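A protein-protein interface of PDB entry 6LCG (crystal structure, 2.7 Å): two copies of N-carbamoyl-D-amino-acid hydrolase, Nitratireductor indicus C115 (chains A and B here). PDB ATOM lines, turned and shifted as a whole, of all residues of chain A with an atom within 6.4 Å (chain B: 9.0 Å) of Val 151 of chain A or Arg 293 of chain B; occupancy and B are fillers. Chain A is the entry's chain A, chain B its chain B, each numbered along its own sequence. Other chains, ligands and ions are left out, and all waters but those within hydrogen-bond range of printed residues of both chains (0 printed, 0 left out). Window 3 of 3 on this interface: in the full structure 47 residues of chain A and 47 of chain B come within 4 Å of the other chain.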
ATOM      1  N   ARG A 106       6.486  27.961  23.123  1.00  0.00           N
ATOM      2  CA  ARG A 106       6.092  26.594  22.822  1.00  0.00           C
ATOM      3  C   ARG A 106       4.989  26.142  23.770  1.00  0.00           C
ATOM      4  O   ARG A 106       4.946  26.541  24.937  1.00  0.00           O
ATOM      5  CB  ARG A 106       7.291  25.647  22.915  1.00  0.00           C
ATOM      6  CG  ARG A 106       8.496  26.115  22.114  1.00  0.00           C
ATOM      7  CD  ARG A 106       9.525  25.012  21.951  1.00  0.00           C
ATOM      8  NE  ARG A 106       9.014  23.913  21.139  1.00  0.00           N
ATOM      9  CZ  ARG A 106       9.715  22.829  20.826  1.00  0.00           C
ATOM     10  NH1 ARG A 106      10.962  22.696  21.258  1.00  0.00           N
ATOM     11  NH2 ARG A 106       9.170  21.876  20.083  1.00  0.00           N
ATOM     12  N   ARG A 107       4.095  25.301  23.252  1.00  0.00           N
ATOM     13  CA  ARG A 107       2.923  24.839  23.984  1.00  0.00           C
ATOM     14  C   ARG A 107       2.897  23.319  23.989  1.00  0.00           C
ATOM     15  O   ARG A 107       2.968  22.690  22.929  1.00  0.00           O
ATOM     16  CB  ARG A 107       1.638  25.392  23.359  1.00  0.00           C
ATOM     17  CG  ARG A 107       1.539  26.905  23.410  1.00  0.00           C
ATOM     18  CD  ARG A 107       0.498  27.439  22.441  1.00  0.00           C
ATOM     19  NE  ARG A 107       0.457  28.898  22.454  1.00  0.00           N
ATOM     20  CZ  ARG A 107       1.317  29.675  21.802  1.00  0.00           C
ATOM     21  NH1 ARG A 107       2.288  29.132  21.080  1.00  0.00           N
ATOM     22  NH2 ARG A 107       1.207  30.994  21.872  1.00  0.00           N
ATOM     23  N   PHE A 108       2.788  22.732  25.178  1.00  0.00           N
ATOM     24  CA  PHE A 108       2.791  21.286  25.331  1.00  0.00           C
ATOM     25  C   PHE A 108       1.646  20.846  26.230  1.00  0.00           C
ATOM     26  O   PHE A 108       1.243  21.562  27.151  1.00  0.00           O
ATOM     27  CB  PHE A 108       4.116  20.778  25.924  1.00  0.00           C
ATOM     28  CG  PHE A 108       5.323  21.100  25.091  1.00  0.00           C
ATOM     29  CD1 PHE A 108       5.611  20.368  23.952  1.00  0.00           C
ATOM     30  CD2 PHE A 108       6.180  22.125  25.458  1.00  0.00           C
ATOM     31  CE1 PHE A 108       6.724  20.659  23.187  1.00  0.00           C
ATOM     32  CE2 PHE A 108       7.295  22.420  24.697  1.00  0.00           C
ATOM     33  CZ  PHE A 108       7.567  21.686  23.560  1.00  0.00           C
ATOM     34  N   ARG A 125       5.793  15.256  28.098  1.00  0.00           N
ATOM     35  CA  ARG A 125       5.004  16.062  27.179  1.00  0.00           C
ATOM     36  C   ARG A 125       4.359  15.153  26.144  1.00  0.00           C
ATOM     37  O   ARG A 125       5.005  14.243  25.615  1.00  0.00           O
ATOM     38  CB  ARG A 125       5.872  17.129  26.505  1.00  0.00           C
ATOM     39  CG  ARG A 125       6.380  18.186  27.474  1.00  0.00           C
ATOM     40  CD  ARG A 125       7.500  19.016  26.879  1.00  0.00           C
ATOM     41  NE  ARG A 125       7.886  20.109  27.766  1.00  0.00           N
ATOM     42  CZ  ARG A 125       8.923  20.913  27.556  1.00  0.00           C
ATOM     43  NH1 ARG A 125       9.689  20.744  26.488  1.00  0.00           N
ATOM     44  NH2 ARG A 125       9.197  21.884  28.415  1.00  0.00           N
ATOM     45  N   LYS A 126       3.081  15.405  25.864  1.00  0.00           N
ATOM     46  CA  LYS A 126       2.283  14.491  25.056  1.00  0.00           C
ATOM     47  C   LYS A 126       2.880  14.320  23.664  1.00  0.00           C
ATOM     48  O   LYS A 126       3.339  15.281  23.040  1.00  0.00           O
ATOM     49  CB  LYS A 126       0.848  15.005  24.956  1.00  0.00           C
ATOM     50  CG  LYS A 126      -0.161  13.976  24.483  1.00  0.00           C
ATOM     51  CD  LYS A 126      -1.566  14.554  24.495  1.00  0.00           C
ATOM     52  CE  LYS A 126      -2.605  13.482  24.232  1.00  0.00           C
ATOM     53  NZ  LYS A 126      -3.988  14.033  24.277  1.00  0.00           N
ATOM     54  N   ILE A 127       2.871  13.080  23.176  1.00  0.00           N
ATOM     55  CA  ILE A 127       3.470  12.748  21.888  1.00  0.00           C
ATOM     56  C   ILE A 127       2.390  12.613  20.823  1.00  0.00           C
ATOM     57  O   ILE A 127       2.433  13.291  19.791  1.00  0.00           O
ATOM     58  CB  ILE A 127       4.311  11.462  21.989  1.00  0.00           C
ATOM     59  CG1 ILE A 127       5.536  11.693  22.875  1.00  0.00           C
ATOM     60  CG2 ILE A 127       4.721  10.982  20.607  1.00  0.00           C
ATOM     61  CD1 ILE A 127       6.442  10.486  22.999  1.00  0.00           C
ATOM     62  N   HIS A 128       1.418  11.737  21.065  1.00  0.00           N
ATOM     63  CA  HIS A 128       0.348  11.469  20.106  1.00  0.00           C
ATOM     64  C   HIS A 128      -0.762  12.491  20.317  1.00  0.00           C
ATOM     65  O   HIS A 128      -1.610  12.332  21.197  1.00  0.00           O
ATOM     66  CB  HIS A 128      -0.175  10.045  20.261  1.00  0.00           C
ATOM     67  CG  HIS A 128       0.891   8.997  20.179  1.00  0.00           C
ATOM     68  ND1 HIS A 128       1.605   8.572  21.279  1.00  0.00           N
ATOM     69  CD2 HIS A 128       1.365   8.288  19.127  1.00  0.00           C
ATOM     70  CE1 HIS A 128       2.472   7.647  20.909  1.00  0.00           C
ATOM     71  NE2 HIS A 128       2.347   7.455  19.609  1.00  0.00           N
ATOM     72  N   LEU A 129      -0.760  13.542  19.506  1.00  0.00           N
ATOM     73  CA  LEU A 129      -1.790  14.569  19.600  1.00  0.00           C
ATOM     74  C   LEU A 129      -3.022  14.138  18.814  1.00  0.00           C
ATOM     75  O   LEU A 129      -2.911  13.851  17.616  1.00  0.00           O
ATOM     76  CB  LEU A 129      -1.267  15.901  19.078  1.00  0.00           C
ATOM     77  CG  LEU A 129      -0.129  16.526  19.887  1.00  0.00           C
ATOM     78  CD1 LEU A 129       0.278  17.870  19.303  1.00  0.00           C
ATOM     79  CD2 LEU A 129      -0.532  16.670  21.346  1.00  0.00           C
ATOM     80  N   PHE A 149      -1.422  22.656  20.629  1.00  0.00           N
ATOM     81  CA  PHE A 149      -0.246  21.993  21.170  1.00  0.00           C
ATOM     82  C   PHE A 149       0.632  21.482  20.039  1.00  0.00           C
ATOM     83  O   PHE A 149       0.149  21.157  18.951  1.00  0.00           O
ATOM     84  CB  PHE A 149      -0.622  20.817  22.085  1.00  0.00           C
ATOM     85  CG  PHE A 149      -1.515  21.195  23.228  1.00  0.00           C
ATOM     86  CD1 PHE A 149      -1.006  21.861  24.331  1.00  0.00           C
ATOM     87  CD2 PHE A 149      -2.861  20.874  23.207  1.00  0.00           C
ATOM     88  CE1 PHE A 149      -1.826  22.206  25.389  1.00  0.00           C
ATOM     89  CE2 PHE A 149      -3.686  21.215  24.261  1.00  0.00           C
ATOM     90  CZ  PHE A 149      -3.168  21.882  25.354  1.00  0.00           C
ATOM     91  N   GLU A 150       1.931  21.416  20.307  1.00  0.00           N
ATOM     92  CA  GLU A 150       2.891  20.786  19.417  1.00  0.00           C
ATOM     93  C   GLU A 150       3.417  19.510  20.061  1.00  0.00           C
ATOM     94  O   GLU A 150       3.276  19.295  21.268  1.00  0.00           O
ATOM     95  CB  GLU A 150       4.043  21.740  19.079  1.00  0.00           C
ATOM     96  CG  GLU A 150       4.559  22.542  20.259  1.00  0.00           C
ATOM     97  CD  GLU A 150       5.450  23.696  19.839  1.00  0.00           C
ATOM     98  OE1 GLU A 150       6.526  23.442  19.259  1.00  0.00           O
ATOM     99  OE2 GLU A 150       5.069  24.861  20.084  1.00  0.00           O
ATOM    100  N   VAL A 151       4.018  18.653  19.231  1.00  0.00           N
ATOM    101  CA  VAL A 151       4.488  17.357  19.706  1.00  0.00           C
ATOM    102  C   VAL A 151       5.559  17.556  20.766  1.00  0.00           C
ATOM    103  O   VAL A 151       6.485  18.361  20.600  1.00  0.00           O
ATOM    104  CB  VAL A 151       5.009  16.515  18.532  1.00  0.00           C
ATOM    105  CG1 VAL A 151       5.498  15.161  19.024  1.00  0.00           C
ATOM    106  CG2 VAL A 151       3.925  16.347  17.478  1.00  0.00           C
ATOM    107  N   GLY A 152       5.434  16.821  21.870  1.00  0.00           N
ATOM    108  CA  GLY A 152       6.388  16.951  22.951  1.00  0.00           C
ATOM    109  C   GLY A 152       7.772  16.471  22.561  1.00  0.00           C
ATOM    110  O   GLY A 152       7.947  15.640  21.669  1.00  0.00           O
ATOM    111  N   ASN A 153       8.775  17.010  23.255  1.00  0.00           N
ATOM    112  CA  ASN A 153      10.175  16.718  22.979  1.00  0.00           C
ATOM    113  C   ASN A 153      10.851  15.975  24.127  1.00  0.00           C
ATOM    114  O   ASN A 153      12.079  16.025  24.258  1.00  0.00           O
ATOM    115  CB  ASN A 153      10.926  18.013  22.665  1.00  0.00           C
ATOM    116  CG  ASN A 153      10.831  19.026  23.788  1.00  0.00           C
ATOM    117  OD1 ASN A 153       9.950  18.940  24.645  1.00  0.00           O
ATOM    118  ND2 ASN A 153      11.737  19.997  23.790  1.00  0.00           N
ATOM    119  N   THR A 304       6.004   4.775   8.818  1.00  0.00           N
ATOM    120  CA  THR A 304       4.894   5.360   9.561  1.00  0.00           C
ATOM    121  C   THR A 304       3.540   4.830   9.121  1.00  0.00           C
ATOM    122  O   THR A 304       2.707   4.498   9.967  1.00  0.00           O
ATOM    123  CB  THR A 304       4.908   6.888   9.419  1.00  0.00           C
ATOM    124  OG1 THR A 304       6.155   7.405   9.900  1.00  0.00           O
ATOM    125  CG2 THR A 304       3.768   7.513  10.210  1.00  0.00           C
ATOM    126  N   ASN B 287      -5.280   5.503  12.225  1.00  0.00           N
ATOM    127  CA  ASN B 287      -4.617   5.896  10.984  1.00  0.00           C
ATOM    128  C   ASN B 287      -3.125   5.999  11.272  1.00  0.00           C
ATOM    129  O   ASN B 287      -2.662   6.974  11.869  1.00  0.00           O
ATOM    130  CB  ASN B 287      -5.181   7.212  10.462  1.00  0.00           C
ATOM    131  CG  ASN B 287      -4.731   7.518   9.047  1.00  0.00           C
ATOM    132  OD1 ASN B 287      -3.609   7.972   8.824  1.00  0.00           O
ATOM    133  ND2 ASN B 287      -5.610   7.275   8.082  1.00  0.00           N
ATOM    134  N   PHE B 288      -2.368   4.983  10.851  1.00  0.00           N
ATOM    135  CA  PHE B 288      -0.948   4.924  11.187  1.00  0.00           C
ATOM    136  C   PHE B 288      -0.174   6.071  10.549  1.00  0.00           C
ATOM    137  O   PHE B 288       0.755   6.617  11.156  1.00  0.00           O
ATOM    138  CB  PHE B 288      -0.361   3.580  10.755  1.00  0.00           C
ATOM    139  CG  PHE B 288      -0.805   2.420  11.601  1.00  0.00           C
ATOM    140  CD1 PHE B 288      -1.465   2.630  12.803  1.00  0.00           C
ATOM    141  CD2 PHE B 288      -0.553   1.119  11.200  1.00  0.00           C
ATOM    142  CE1 PHE B 288      -1.871   1.562  13.582  1.00  0.00           C
ATOM    143  CE2 PHE B 288      -0.955   0.048  11.976  1.00  0.00           C
ATOM    144  CZ  PHE B 288      -1.614   0.271  13.168  1.00  0.00           C
ATOM    145  N   ALA B 289      -0.541   6.454   9.324  1.00  0.00           N
ATOM    146  CA  ALA B 289       0.186   7.511   8.630  1.00  0.00           C
ATOM    147  C   ALA B 289       0.005   8.868   9.303  1.00  0.00           C
ATOM    148  O   ALA B 289       0.866   9.745   9.162  1.00  0.00           O
ATOM    149  CB  ALA B 289      -0.262   7.581   7.170  1.00  0.00           C
ATOM    150  N   ALA B 290      -1.089   9.059  10.040  1.00  0.00           N
ATOM    151  CA  ALA B 290      -1.396  10.363  10.612  1.00  0.00           C
ATOM    152  C   ALA B 290      -0.811  10.536  12.011  1.00  0.00           C
ATOM    153  O   ALA B 290      -0.164  11.550  12.295  1.00  0.00           O
ATOM    154  CB  ALA B 290      -2.914  10.574  10.643  1.00  0.00           C
ATOM    155  N   HIS B 291      -1.004   9.550  12.885  1.00  0.00           N
ATOM    156  CA  HIS B 291      -0.707   9.720  14.302  1.00  0.00           C
ATOM    157  C   HIS B 291       0.613   9.105  14.747  1.00  0.00           C
ATOM    158  O   HIS B 291       1.246   9.644  15.660  1.00  0.00           O
ATOM    159  CB  HIS B 291      -1.833   9.120  15.147  1.00  0.00           C
ATOM    160  CG  HIS B 291      -3.196   9.597  14.760  1.00  0.00           C
ATOM    161  ND1 HIS B 291      -3.838   9.166  13.620  1.00  0.00           N
ATOM    162  CD2 HIS B 291      -4.037  10.472  15.359  1.00  0.00           C
ATOM    163  CE1 HIS B 291      -5.018   9.754  13.535  1.00  0.00           C
ATOM    164  NE2 HIS B 291      -5.164  10.549  14.580  1.00  0.00           N
ATOM    165  N   ARG B 292       1.042   7.994  14.150  1.00  0.00           N
ATOM    166  CA  ARG B 292       2.235   7.309  14.637  1.00  0.00           C
ATOM    167  C   ARG B 292       3.471   8.189  14.517  1.00  0.00           C
ATOM    168  O   ARG B 292       3.714   8.802  13.477  1.00  0.00           O
ATOM    169  CB  ARG B 292       2.445   6.002  13.877  1.00  0.00           C
ATOM    170  CG  ARG B 292       1.522   4.892  14.326  1.00  0.00           C
ATOM    171  CD  ARG B 292       1.820   3.588  13.614  1.00  0.00           C
ATOM    172  NE  ARG B 292       2.921   2.855  14.231  1.00  0.00           N
ATOM    173  CZ  ARG B 292       4.169   2.845  13.773  1.00  0.00           C
ATOM    174  NH1 ARG B 292       4.489   3.532  12.683  1.00  0.00           N
ATOM    175  NH2 ARG B 292       5.097   2.144  14.407  1.00  0.00           N
ATOM    176  N   ARG B 293       4.255   8.243  15.597  1.00  0.00           N
ATOM    177  CA  ARG B 293       5.496   9.011  15.661  1.00  0.00           C
ATOM    178  C   ARG B 293       6.649   8.033  15.855  1.00  0.00           C
ATOM    179  O   ARG B 293       7.086   7.791  16.991  1.00  0.00           O
ATOM    180  CB  ARG B 293       5.459  10.039  16.789  1.00  0.00           C
ATOM    181  CG  ARG B 293       4.224  10.922  16.793  1.00  0.00           C
ATOM    182  CD  ARG B 293       4.221  11.884  15.621  1.00  0.00           C
ATOM    183  NE  ARG B 293       5.438  12.689  15.583  1.00  0.00           N
ATOM    184  CZ  ARG B 293       5.560  13.830  14.914  1.00  0.00           C
ATOM    185  NH1 ARG B 293       4.534  14.313  14.228  1.00  0.00           N
ATOM    186  NH2 ARG B 293       6.708  14.492  14.938  1.00  0.00           N
ATOM    187  N   PRO B 294       7.177   7.462  14.769  1.00  0.00           N
ATOM    188  CA  PRO B 294       8.224   6.435  14.904  1.00  0.00           C
ATOM    189  C   PRO B 294       9.528   6.946  15.497  1.00  0.00           C
ATOM    190  O   PRO B 294      10.360   6.122  15.898  1.00  0.00           O
ATOM    191  CB  PRO B 294       8.425   5.949  13.464  1.00  0.00           C
ATOM    192  CG  PRO B 294       7.983   7.097  12.617  1.00  0.00           C
ATOM    193  CD  PRO B 294       6.855   7.748  13.361  1.00  0.00           C
ATOM    194  N   GLU B 295       9.737   8.263  15.572  1.00  0.00           N
ATOM    195  CA  GLU B 295      10.973   8.785  16.143  1.00  0.00           C
ATOM    196  C   GLU B 295      11.048   8.601  17.654  1.00  0.00           C
ATOM    197  O   GLU B 295      12.117   8.822  18.234  1.00  0.00           O
ATOM    198  CB  GLU B 295      11.137  10.267  15.793  1.00  0.00           C
ATOM    199  CG  GLU B 295      10.161  11.204  16.493  1.00  0.00           C
ATOM    200  CD  GLU B 295       8.828  11.323  15.776  1.00  0.00           C
ATOM    201  OE1 GLU B 295       8.552  10.501  14.877  1.00  0.00           O
ATOM    202  OE2 GLU B 295       8.056  12.247  16.110  1.00  0.00           O
ATOM    203  N   PHE B 296       9.952   8.206  18.300  1.00  0.00           N
ATOM    204  CA  PHE B 296       9.940   7.926  19.728  1.00  0.00           C
ATOM    205  C   PHE B 296       9.846   6.439  20.039  1.00  0.00           C
ATOM    206  O   PHE B 296       9.805   6.069  21.217  1.00  0.00           O
ATOM    207  CB  PHE B 296       8.780   8.665  20.407  1.00  0.00           C
ATOM    208  CG  PHE B 296       8.882  10.161  20.326  1.00  0.00           C
ATOM    209  CD1 PHE B 296       9.736  10.856  21.166  1.00  0.00           C
ATOM    210  CD2 PHE B 296       8.119  10.873  19.416  1.00  0.00           C
ATOM    211  CE1 PHE B 296       9.831  12.233  21.097  1.00  0.00           C
ATOM    212  CE2 PHE B 296       8.210  12.250  19.342  1.00  0.00           C
ATOM    213  CZ  PHE B 296       9.068  12.931  20.184  1.00  0.00           C
ATOM    214  N   TYR B 297       9.811   5.580  19.022  1.00  0.00           N
ATOM    215  CA  TYR B 297       9.683   4.142  19.215  1.00  0.00           C
ATOM    216  C   TYR B 297      11.006   3.408  19.037  1.00  0.00           C
ATOM    217  O   TYR B 297      11.010   2.179  18.927  1.00  0.00           O
ATOM    218  CB  TYR B 297       8.648   3.560  18.244  1.00  0.00           C
ATOM    219  CG  TYR B 297       7.315   4.281  18.183  1.00  0.00           C
ATOM    220  CD1 TYR B 297       6.839   5.022  19.258  1.00  0.00           C
ATOM    221  CD2 TYR B 297       6.526   4.207  17.041  1.00  0.00           C
ATOM    222  CE1 TYR B 297       5.621   5.677  19.192  1.00  0.00           C
ATOM    223  CE2 TYR B 297       5.310   4.855  16.966  1.00  0.00           C
ATOM    224  CZ  TYR B 297       4.861   5.588  18.043  1.00  0.00           C
ATOM    225  OH  TYR B 297       3.647   6.232  17.967  1.00  0.00           O
ATOM    226  N   GLN B 298      12.128   4.133  19.016  1.00  0.00           N
ATOM    227  CA  GLN B 298      13.402   3.540  18.625  1.00  0.00           C
ATOM    228  C   GLN B 298      13.865   2.438  19.570  1.00  0.00           C
ATOM    229  O   GLN B 298      14.640   1.571  19.152  1.00  0.00           O
ATOM    230  CB  GLN B 298      14.476   4.625  18.528  1.00  0.00           C
ATOM    231  CG  GLN B 298      14.235   5.621  17.409  1.00  0.00           C
ATOM    232  CD  GLN B 298      14.165   4.957  16.046  1.00  0.00           C
ATOM    233  OE1 GLN B 298      14.926   4.034  15.753  1.00  0.00           O
ATOM    234  NE2 GLN B 298      13.245   5.420  15.209  1.00  0.00           N
ATOM    235  N   ILE B 300      12.162   0.016  20.583  1.00  0.00           N
ATOM    236  CA  ILE B 300      11.521  -1.244  20.215  1.00  0.00           C
ATOM    237  C   ILE B 300      12.435  -2.074  19.319  1.00  0.00           C
ATOM    238  O   ILE B 300      12.458  -3.308  19.406  1.00  0.00           O
ATOM    239  CB  ILE B 300      10.158  -0.972  19.550  1.00  0.00           C
ATOM    240  CG1 ILE B 300       9.215  -0.288  20.541  1.00  0.00           C
ATOM    241  CG2 ILE B 300       9.537  -2.260  19.028  1.00  0.00           C
ATOM    242  CD1 ILE B 300       7.854   0.028  19.973  1.00  0.00           C
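NE2 of His 128 of chain A sits at hydrogen-bond distance from OH of Tyr 297 of chain B, at 2.4 Å.
O of Thr 304 of chain A sits at hydrogen-bond distance from NH1 of Arg 292 of chain B (3.4 Å).
The backbone carbonyl oxygen of Thr 304 of chain A lies close to the backbone carbonyl oxygen of Phe 288 of chain B (3.1 Å).
O of Lys 126 of chain A sits at hydrogen-bond distance from N of Gly 152 of chain A (2.9 Å).
The backbone NH of Ala 289 of chain B lies close to the side-chain amide oxygen of Asn 287 of chain B, at 3.5 Å.
O of Asn 287 of chain B sits at hydrogen-bond distance from ND1 of His 291 of chain B (3.0 Å).
The guanidinium group of Arg 293 of chain B is in salt-bridge range of the side-chain carboxylate of Glu 295 of chain B (2.7 Å).
OH of Tyr 297 of chain B lies within hydrogen-bond range of N of Arg 293 of chain B (3.2 Å).
The side-chain amide nitrogen of Gln 298 of chain B lies within hydrogen-bond range of the backbone carbonyl oxygen of Pro 294 of chain B (3.0 Å).
Among the printed residues, merely in contact across the chains: Ile 127 of chain A with Arg 293 of chain B, Ile 127 of chain A with Phe 296 of chain B, His 128 of chain A with His 291 of chain B, Val 151 of chain A with Arg 293 of chain B, Val 151 of chain A with Phe 296 of chain B, Gly 152 of chain A with Phe 296 of chain B, Thr 304 of chain A with Ala 289 of chain B and Thr 304 of chain A with Pro 294 of chain B.
Arg 106 of chain A touches none of the printed residues of chain B.
Printed residues of chain B within 4 Å of Ile 127 of chain A: Arg 293 and Phe 296.
Printed residues of chain B within 4 Å of His 128 of chain A: His 291 (3.7 Å) and Tyr 297 (2.4 Å).
Printed residues of chain B within 4 Å of Val 151 of chain A: Arg 293 (3.9 Å) and Phe 296 (3.99 Å).
Gly 152 of chain A touches one residue of chain B.
Of the printed residues of chain A, Phe 288 of chain B touches Thr 304 (3.1 Å).
Printed residues of chain A within 4 Å of His 291 of chain B: His 128.
Arg 293 of chain B touches two residues of chain A.
Of the printed residues of chain A, Pro 294 of chain B touches Thr 304.
The nearest residue of chain A that does not touch Arg 293 of chain B is His 128 of chain A (4.5 Å).
The nearest printed residue of chain A that does not touch Ala 289 of chain B is His 128 of chain A (9.9 Å).
Hydrophobic or aromatic side chains of chain B that line the printed part of chain A: Phe 288, Pro 294, Phe 296 and Tyr 297.
Hydrophobic or aromatic side chains of chain A that line the printed part of chain B: Ile 127, His 128 and Val 151.
No position is printed for both chains.
Of the 11 pairs that touch across the chains among the printed residues, none has its exchanged pair printed and touching as well.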
